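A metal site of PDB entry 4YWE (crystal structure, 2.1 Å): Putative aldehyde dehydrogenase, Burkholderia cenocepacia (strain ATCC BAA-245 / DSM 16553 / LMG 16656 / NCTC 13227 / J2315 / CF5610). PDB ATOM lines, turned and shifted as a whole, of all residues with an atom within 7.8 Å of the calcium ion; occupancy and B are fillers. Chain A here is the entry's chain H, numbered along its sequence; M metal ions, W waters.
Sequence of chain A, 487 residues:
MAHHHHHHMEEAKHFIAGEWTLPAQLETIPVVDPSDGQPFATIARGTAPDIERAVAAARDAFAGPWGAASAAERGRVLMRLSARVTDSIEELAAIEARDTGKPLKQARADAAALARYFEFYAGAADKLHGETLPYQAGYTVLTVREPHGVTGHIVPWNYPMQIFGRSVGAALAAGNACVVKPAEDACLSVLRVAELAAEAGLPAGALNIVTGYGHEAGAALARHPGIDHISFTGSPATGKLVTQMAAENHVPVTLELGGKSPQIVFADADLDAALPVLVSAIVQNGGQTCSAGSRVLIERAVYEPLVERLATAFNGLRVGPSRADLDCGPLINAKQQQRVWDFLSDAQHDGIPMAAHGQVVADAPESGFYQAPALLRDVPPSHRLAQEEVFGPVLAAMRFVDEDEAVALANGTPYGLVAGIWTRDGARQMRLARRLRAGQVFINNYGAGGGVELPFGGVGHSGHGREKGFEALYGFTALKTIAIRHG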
ATOM      1  N   PRO A  30      -4.646 -15.771 -19.391  1.00  0.00           N
ATOM      2  CA  PRO A  30      -4.394 -14.619 -20.272  1.00  0.00           C
ATOM      3  C   PRO A  30      -4.264 -15.011 -21.744  1.00  0.00           C
ATOM      4  O   PRO A  30      -3.771 -16.096 -22.055  1.00  0.00           O
ATOM      5  CB  PRO A  30      -3.069 -14.050 -19.752  1.00  0.00           C
ATOM      6  CG  PRO A  30      -2.923 -14.614 -18.375  1.00  0.00           C
ATOM      7  CD  PRO A  30      -3.548 -15.964 -18.423  1.00  0.00           C
ATOM      8  N   VAL A  31      -4.717 -14.130 -22.638  1.00  0.00           N
ATOM      9  CA  VAL A  31      -4.563 -14.344 -24.076  1.00  0.00           C
ATOM     10  C   VAL A  31      -3.521 -13.376 -24.609  1.00  0.00           C
ATOM     11  O   VAL A  31      -3.652 -12.163 -24.474  1.00  0.00           O
ATOM     12  CB  VAL A  31      -5.905 -14.170 -24.813  1.00  0.00           C
ATOM     13  CG1 VAL A  31      -5.710 -14.352 -26.311  1.00  0.00           C
ATOM     14  CG2 VAL A  31      -6.940 -15.145 -24.281  1.00  0.00           C
ATOM     15  N   VAL A  32      -2.470 -13.924 -25.226  1.00  0.00           N
ATOM     16  CA  VAL A  32      -1.335 -13.109 -25.648  1.00  0.00           C
ATOM     17  C   VAL A  32      -1.269 -12.982 -27.170  1.00  0.00           C
ATOM     18  O   VAL A  32      -1.418 -13.957 -27.895  1.00  0.00           O
ATOM     19  CB  VAL A  32      -0.023 -13.701 -25.092  1.00  0.00           C
ATOM     20  CG1 VAL A  32       1.184 -12.942 -25.642  1.00  0.00           C
ATOM     21  CG2 VAL A  32      -0.025 -13.672 -23.571  1.00  0.00           C
ATOM     22  N   ASP A  33      -1.033 -11.762 -27.638  1.00  0.00           N
ATOM     23  CA  ASP A  33      -0.784 -11.490 -29.053  1.00  0.00           C
ATOM     24  C   ASP A  33       0.696 -11.697 -29.358  1.00  0.00           C
ATOM     25  O   ASP A  33       1.528 -10.913 -28.896  1.00  0.00           O
ATOM     26  CB  ASP A  33      -1.231 -10.072 -29.416  1.00  0.00           C
ATOM     27  CG  ASP A  33      -1.160  -9.786 -30.914  1.00  0.00           C
ATOM     28  OD1 ASP A  33      -0.529 -10.565 -31.662  1.00  0.00           O
ATOM     29  OD2 ASP A  33      -1.744  -8.783 -31.348  1.00  0.00           O
ATOM     30  N   PRO A  34       1.025 -12.736 -30.135  1.00  0.00           N
ATOM     31  CA  PRO A  34       2.411 -13.080 -30.467  1.00  0.00           C
ATOM     32  C   PRO A  34       3.141 -11.997 -31.243  1.00  0.00           C
ATOM     33  O   PRO A  34       4.376 -12.019 -31.314  1.00  0.00           O
ATOM     34  CB  PRO A  34       2.265 -14.353 -31.306  1.00  0.00           C
ATOM     35  CG  PRO A  34       0.913 -14.880 -30.989  1.00  0.00           C
ATOM     36  CD  PRO A  34       0.070 -13.680 -30.727  1.00  0.00           C
ATOM     37  N   GLN A  38       1.991  -9.344 -25.890  1.00  0.00           N
ATOM     38  CA  GLN A  38       1.271  -8.618 -24.845  1.00  0.00           C
ATOM     39  C   GLN A  38      -0.185  -9.073 -24.748  1.00  0.00           C
ATOM     40  O   GLN A  38      -0.849  -9.279 -25.775  1.00  0.00           O
ATOM     41  CB  GLN A  38       1.347  -7.119 -25.116  1.00  0.00           C
ATOM     42  CG  GLN A  38       2.756  -6.581 -25.270  1.00  0.00           C
ATOM     43  CD  GLN A  38       3.525  -6.539 -23.967  1.00  0.00           C
ATOM     44  OE1 GLN A  38       4.543  -7.206 -23.825  1.00  0.00           O
ATOM     45  NE2 GLN A  38       3.048  -5.740 -23.010  1.00  0.00           N
ATOM     46  N   PHE A  40      -4.203  -9.163 -24.273  1.00  0.00           N
ATOM     47  CA  PHE A  40      -5.275  -8.291 -24.745  1.00  0.00           C
ATOM     48  C   PHE A  40      -6.650  -8.853 -24.398  1.00  0.00           C
ATOM     49  O   PHE A  40      -7.657  -8.172 -24.548  1.00  0.00           O
ATOM     50  CB  PHE A  40      -5.167  -8.052 -26.258  1.00  0.00           C
ATOM     51  CG  PHE A  40      -5.432  -9.284 -27.080  1.00  0.00           C
ATOM     52  CD1 PHE A  40      -4.424 -10.208 -27.337  1.00  0.00           C
ATOM     53  CD2 PHE A  40      -6.689  -9.513 -27.627  1.00  0.00           C
ATOM     54  CE1 PHE A  40      -4.668 -11.337 -28.094  1.00  0.00           C
ATOM     55  CE2 PHE A  40      -6.939 -10.630 -28.395  1.00  0.00           C
ATOM     56  CZ  PHE A  40      -5.931 -11.543 -28.633  1.00  0.00           C
ATOM     57  N   ILE A  95      -9.393 -12.174 -35.719  1.00  0.00           N
ATOM     58  CA  ILE A  95      -9.259 -12.853 -34.442  1.00  0.00           C
ATOM     59  C   ILE A  95      -8.124 -13.881 -34.503  1.00  0.00           C
ATOM     60  O   ILE A  95      -7.255 -13.911 -33.636  1.00  0.00           O
ATOM     61  CB  ILE A  95     -10.576 -13.538 -34.021  1.00  0.00           C
ATOM     62  CG1 ILE A  95     -11.706 -12.503 -33.964  1.00  0.00           C
ATOM     63  CG2 ILE A  95     -10.415 -14.231 -32.685  1.00  0.00           C
ATOM     64  CD1 ILE A  95     -11.460 -11.378 -32.995  1.00  0.00           C
ATOM     65  N   GLU A  96      -8.148 -14.710 -35.530  1.00  0.00           N
ATOM     66  CA  GLU A  96      -7.170 -15.789 -35.690  1.00  0.00           C
ATOM     67  C   GLU A  96      -5.756 -15.244 -35.849  1.00  0.00           C
ATOM     68  O   GLU A  96      -4.817 -15.745 -35.225  1.00  0.00           O
ATOM     69  CB  GLU A  96      -7.530 -16.662 -36.887  1.00  0.00           C
ATOM     70  CG  GLU A  96      -6.750 -17.968 -36.961  1.00  0.00           C
ATOM     71  CD  GLU A  96      -7.321 -19.051 -36.051  1.00  0.00           C
ATOM     72  OE1 GLU A  96      -7.436 -18.814 -34.836  1.00  0.00           O
ATOM     73  OE2 GLU A  96      -7.663 -20.135 -36.566  1.00  0.00           O
ATOM     74  N   ALA A  97      -5.606 -14.224 -36.687  1.00  0.00           N
ATOM     75  CA  ALA A  97      -4.303 -13.639 -36.964  1.00  0.00           C
ATOM     76  C   ALA A  97      -3.691 -12.999 -35.714  1.00  0.00           C
ATOM     77  O   ALA A  97      -2.488 -13.087 -35.486  1.00  0.00           O
ATOM     78  CB  ALA A  97      -4.414 -12.611 -38.073  1.00  0.00           C
ATOM     79  N   ARG A  98      -4.527 -12.353 -34.911  1.00  0.00           N
ATOM     80  CA  ARG A  98      -4.069 -11.681 -33.704  1.00  0.00           C
ATOM     81  C   ARG A  98      -3.699 -12.693 -32.620  1.00  0.00           C
ATOM     82  O   ARG A  98      -2.773 -12.475 -31.841  1.00  0.00           O
ATOM     83  CB  ARG A  98      -5.145 -10.727 -33.192  1.00  0.00           C
ATOM     84  CG  ARG A  98      -4.700  -9.836 -32.046  1.00  0.00           C
ATOM     85  CD  ARG A  98      -5.816  -8.910 -31.610  1.00  0.00           C
ATOM     86  NE  ARG A  98      -5.383  -7.951 -30.600  1.00  0.00           N
ATOM     87  CZ  ARG A  98      -6.189  -7.119 -29.958  1.00  0.00           C
ATOM     88  NH1 ARG A  98      -7.497  -7.134 -30.215  1.00  0.00           N
ATOM     89  NH2 ARG A  98      -5.707  -6.280 -29.050  1.00  0.00           N
ATOM     90  N   ASP A  99      -4.439 -13.802 -32.603  1.00  0.00           N
ATOM     91  CA  ASP A  99      -4.320 -14.794 -31.540  1.00  0.00           C
ATOM     92  C   ASP A  99      -3.224 -15.826 -31.829  1.00  0.00           C
ATOM     93  O   ASP A  99      -2.538 -16.278 -30.910  1.00  0.00           O
ATOM     94  CB  ASP A  99      -5.668 -15.490 -31.348  1.00  0.00           C
ATOM     95  CG  ASP A  99      -5.737 -16.314 -30.082  1.00  0.00           C
ATOM     96  OD1 ASP A  99      -4.920 -16.073 -29.161  1.00  0.00           O
ATOM     97  OD2 ASP A  99      -6.626 -17.194 -29.993  1.00  0.00           O
ATOM     98  N   THR A 100      -3.045 -16.179 -33.097  1.00  0.00           N
ATOM     99  CA  THR A 100      -2.063 -17.182 -33.479  1.00  0.00           C
ATOM    100  C   THR A 100      -0.766 -16.547 -33.990  1.00  0.00           C
ATOM    101  O   THR A 100       0.308 -17.126 -33.862  1.00  0.00           O
ATOM    102  CB  THR A 100      -2.603 -18.123 -34.571  1.00  0.00           C
ATOM    103  OG1 THR A 100      -2.896 -17.372 -35.756  1.00  0.00           O
ATOM    104  CG2 THR A 100      -3.860 -18.825 -34.105  1.00  0.00           C
ATOM    105  N   GLY A 101      -0.884 -15.358 -34.580  1.00  0.00           N
ATOM    106  CA  GLY A 101       0.277 -14.649 -35.085  1.00  0.00           C
ATOM    107  C   GLY A 101       0.447 -14.734 -36.586  1.00  0.00           C
ATOM    108  O   GLY A 101       1.238 -13.991 -37.167  1.00  0.00           O
ATOM    109  N   TRP A 157      -3.074 -25.073 -31.297  1.00  0.00           N
ATOM    110  CA  TRP A 157      -3.021 -23.618 -31.436  1.00  0.00           C
ATOM    111  C   TRP A 157      -2.588 -23.150 -32.821  1.00  0.00           C
ATOM    112  O   TRP A 157      -2.726 -21.972 -33.143  1.00  0.00           O
ATOM    113  CB  TRP A 157      -2.067 -23.025 -30.385  1.00  0.00           C
ATOM    114  CG  TRP A 157      -0.757 -23.754 -30.295  1.00  0.00           C
ATOM    115  CD1 TRP A 157      -0.386 -24.668 -29.348  1.00  0.00           C
ATOM    116  CD2 TRP A 157       0.366 -23.626 -31.183  1.00  0.00           C
ATOM    117  NE1 TRP A 157       0.885 -25.124 -29.591  1.00  0.00           N
ATOM    118  CE2 TRP A 157       1.377 -24.494 -30.709  1.00  0.00           C
ATOM    119  CE3 TRP A 157       0.621 -22.865 -32.323  1.00  0.00           C
ATOM    120  CZ2 TRP A 157       2.604 -24.621 -31.341  1.00  0.00           C
ATOM    121  CZ3 TRP A 157       1.848 -22.992 -32.955  1.00  0.00           C
ATOM    122  CH2 TRP A 157       2.820 -23.863 -32.463  1.00  0.00           C
ATOM    123  N   ALA A 183      -6.842 -25.112 -27.683  1.00  0.00           N
ATOM    124  CA  ALA A 183      -5.538 -24.808 -27.086  1.00  0.00           C
ATOM    125  C   ALA A 183      -5.538 -23.485 -26.320  1.00  0.00           C
ATOM    126  O   ALA A 183      -6.159 -22.509 -26.753  1.00  0.00           O
ATOM    127  CB  ALA A 183      -4.470 -24.796 -28.155  1.00  0.00           C
ATOM    128  N   GLU A 184      -4.832 -23.458 -25.198  1.00  0.00           N
ATOM    129  CA  GLU A 184      -4.790 -22.279 -24.346  1.00  0.00           C
ATOM    130  C   GLU A 184      -3.916 -21.167 -24.934  1.00  0.00           C
ATOM    131  O   GLU A 184      -3.960 -20.029 -24.459  1.00  0.00           O
ATOM    132  CB  GLU A 184      -4.292 -22.650 -22.944  1.00  0.00           C
ATOM    133  CG  GLU A 184      -2.904 -23.274 -22.904  1.00  0.00           C
ATOM    134  CD  GLU A 184      -2.925 -24.784 -23.088  1.00  0.00           C
ATOM    135  OE1 GLU A 184      -3.795 -25.291 -23.828  1.00  0.00           O
ATOM    136  OE2 GLU A 184      -2.070 -25.472 -22.493  1.00  0.00           O
ATOM    137  N   ASP A 185      -3.128 -21.488 -25.944  1.00  0.00           N
ATOM    138  CA  ASP A 185      -2.284 -20.478 -26.583  1.00  0.00           C
ATOM    139  C   ASP A 185      -3.045 -19.727 -27.669  1.00  0.00           C
ATOM    140  O   ASP A 185      -2.676 -18.613 -28.033  1.00  0.00           O
ATOM    141  CB  ASP A 185      -1.028 -21.118 -27.174  1.00  0.00           C
ATOM    142  CG  ASP A 185       0.029 -21.396 -26.122  1.00  0.00           C
ATOM    143  OD1 ASP A 185       0.753 -20.454 -25.733  1.00  0.00           O
ATOM    144  OD2 ASP A 185       0.135 -22.564 -25.678  1.00  0.00           O
ATOM    145  N   ALA A 186      -4.109 -20.348 -28.186  1.00  0.00           N
ATOM    146  CA  ALA A 186      -4.939 -19.729 -29.210  1.00  0.00           C
ATOM    147  C   ALA A 186      -6.266 -20.470 -29.362  1.00  0.00           C
ATOM    148  O   ALA A 186      -6.289 -21.624 -29.782  1.00  0.00           O
ATOM    149  CB  ALA A 186      -4.211 -19.676 -30.547  1.00  0.00           C
ATOM    150  N   CYS A 187      -7.370 -19.808 -29.019  1.00  0.00           N
ATOM    151  CA  CYS A 187      -8.681 -20.443 -29.082  1.00  0.00           C
ATOM    152  C   CYS A 187      -9.825 -19.438 -29.168  1.00  0.00           C
ATOM    153  O   CYS A 187     -10.989 -19.807 -29.026  1.00  0.00           O
ATOM    154  CB  CYS A 187      -8.895 -21.347 -27.878  1.00  0.00           C
ATOM    155  SG  CYS A 187      -9.034 -20.490 -26.288  1.00  0.00           S
ATOM    156  N   LEU A 188      -9.499 -18.169 -29.408  1.00  0.00           N
ATOM    157  CA  LEU A 188     -10.523 -17.126 -29.442  1.00  0.00           C
ATOM    158  C   LEU A 188     -11.441 -17.257 -30.660  1.00  0.00           C
ATOM    159  O   LEU A 188     -12.645 -17.064 -30.557  1.00  0.00           O
ATOM    160  CB  LEU A 188      -9.879 -15.744 -29.433  1.00  0.00           C
ATOM    161  CG  LEU A 188      -9.285 -15.273 -28.098  1.00  0.00           C
ATOM    162  CD1 LEU A 188      -8.819 -13.823 -28.198  1.00  0.00           C
ATOM    163  CD2 LEU A 188     -10.298 -15.440 -26.968  1.00  0.00           C
ATOM    164  N   ILE A 332       4.209 -18.788 -31.986  1.00  0.00           N
ATOM    165  CA  ILE A 332       3.067 -18.690 -31.081  1.00  0.00           C
ATOM    166  C   ILE A 332       3.444 -18.125 -29.712  1.00  0.00           C
ATOM    167  O   ILE A 332       2.697 -17.346 -29.138  1.00  0.00           O
ATOM    168  CB  ILE A 332       2.358 -20.058 -30.955  1.00  0.00           C
ATOM    169  CG1 ILE A 332       1.035 -19.901 -30.201  1.00  0.00           C
ATOM    170  CG2 ILE A 332       3.252 -21.098 -30.286  1.00  0.00           C
ATOM    171  CD1 ILE A 332       0.089 -18.900 -30.837  1.00  0.00           C
ATOM    172  N   ASN A 333       4.606 -18.507 -29.191  1.00  0.00           N
ATOM    173  CA  ASN A 333       5.063 -18.001 -27.896  1.00  0.00           C
ATOM    174  C   ASN A 333       6.578 -18.104 -27.753  1.00  0.00           C
ATOM    175  O   ASN A 333       7.269 -18.582 -28.660  1.00  0.00           O
ATOM    176  CB  ASN A 333       4.370 -18.738 -26.745  1.00  0.00           C
ATOM    177  CG  ASN A 333       4.467 -20.251 -26.856  1.00  0.00           C
ATOM    178  OD1 ASN A 333       5.459 -20.782 -27.374  1.00  0.00           O
ATOM    179  ND2 ASN A 333       3.457 -20.946 -26.373  1.00  0.00           N
HETATM  180 CA    CA M   1      -2.551 -16.183 -28.441  1.00  0.00          CA
HETATM  181  O   HOH W   1      -2.661 -16.585 -25.847  1.00  0.00           O
HETATM  182  O   HOH W   2      -0.124 -16.619 -28.419  1.00  0.00           O
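The calcium ion is bound by water W2, the backbone carbonyl oxygen of Asp 185, the backbone carbonyl oxygen of Asp 99, the side-chain carboxylate of Asp 99, the backbone carbonyl oxygen of Val 32 and water W1. The calcium ion has six donor atoms within binding distance.
OD2 of Asp 99 is in hydrogen-bond range of N of Cys 187 (2.9 Å). OD1 of Asp 185 lies within hydrogen-bond range of ND2 of Asn 333 (2.8 Å). OD2 of Asp 99 is in hydrogen-bond range of N of Leu 188 (3.1 Å).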
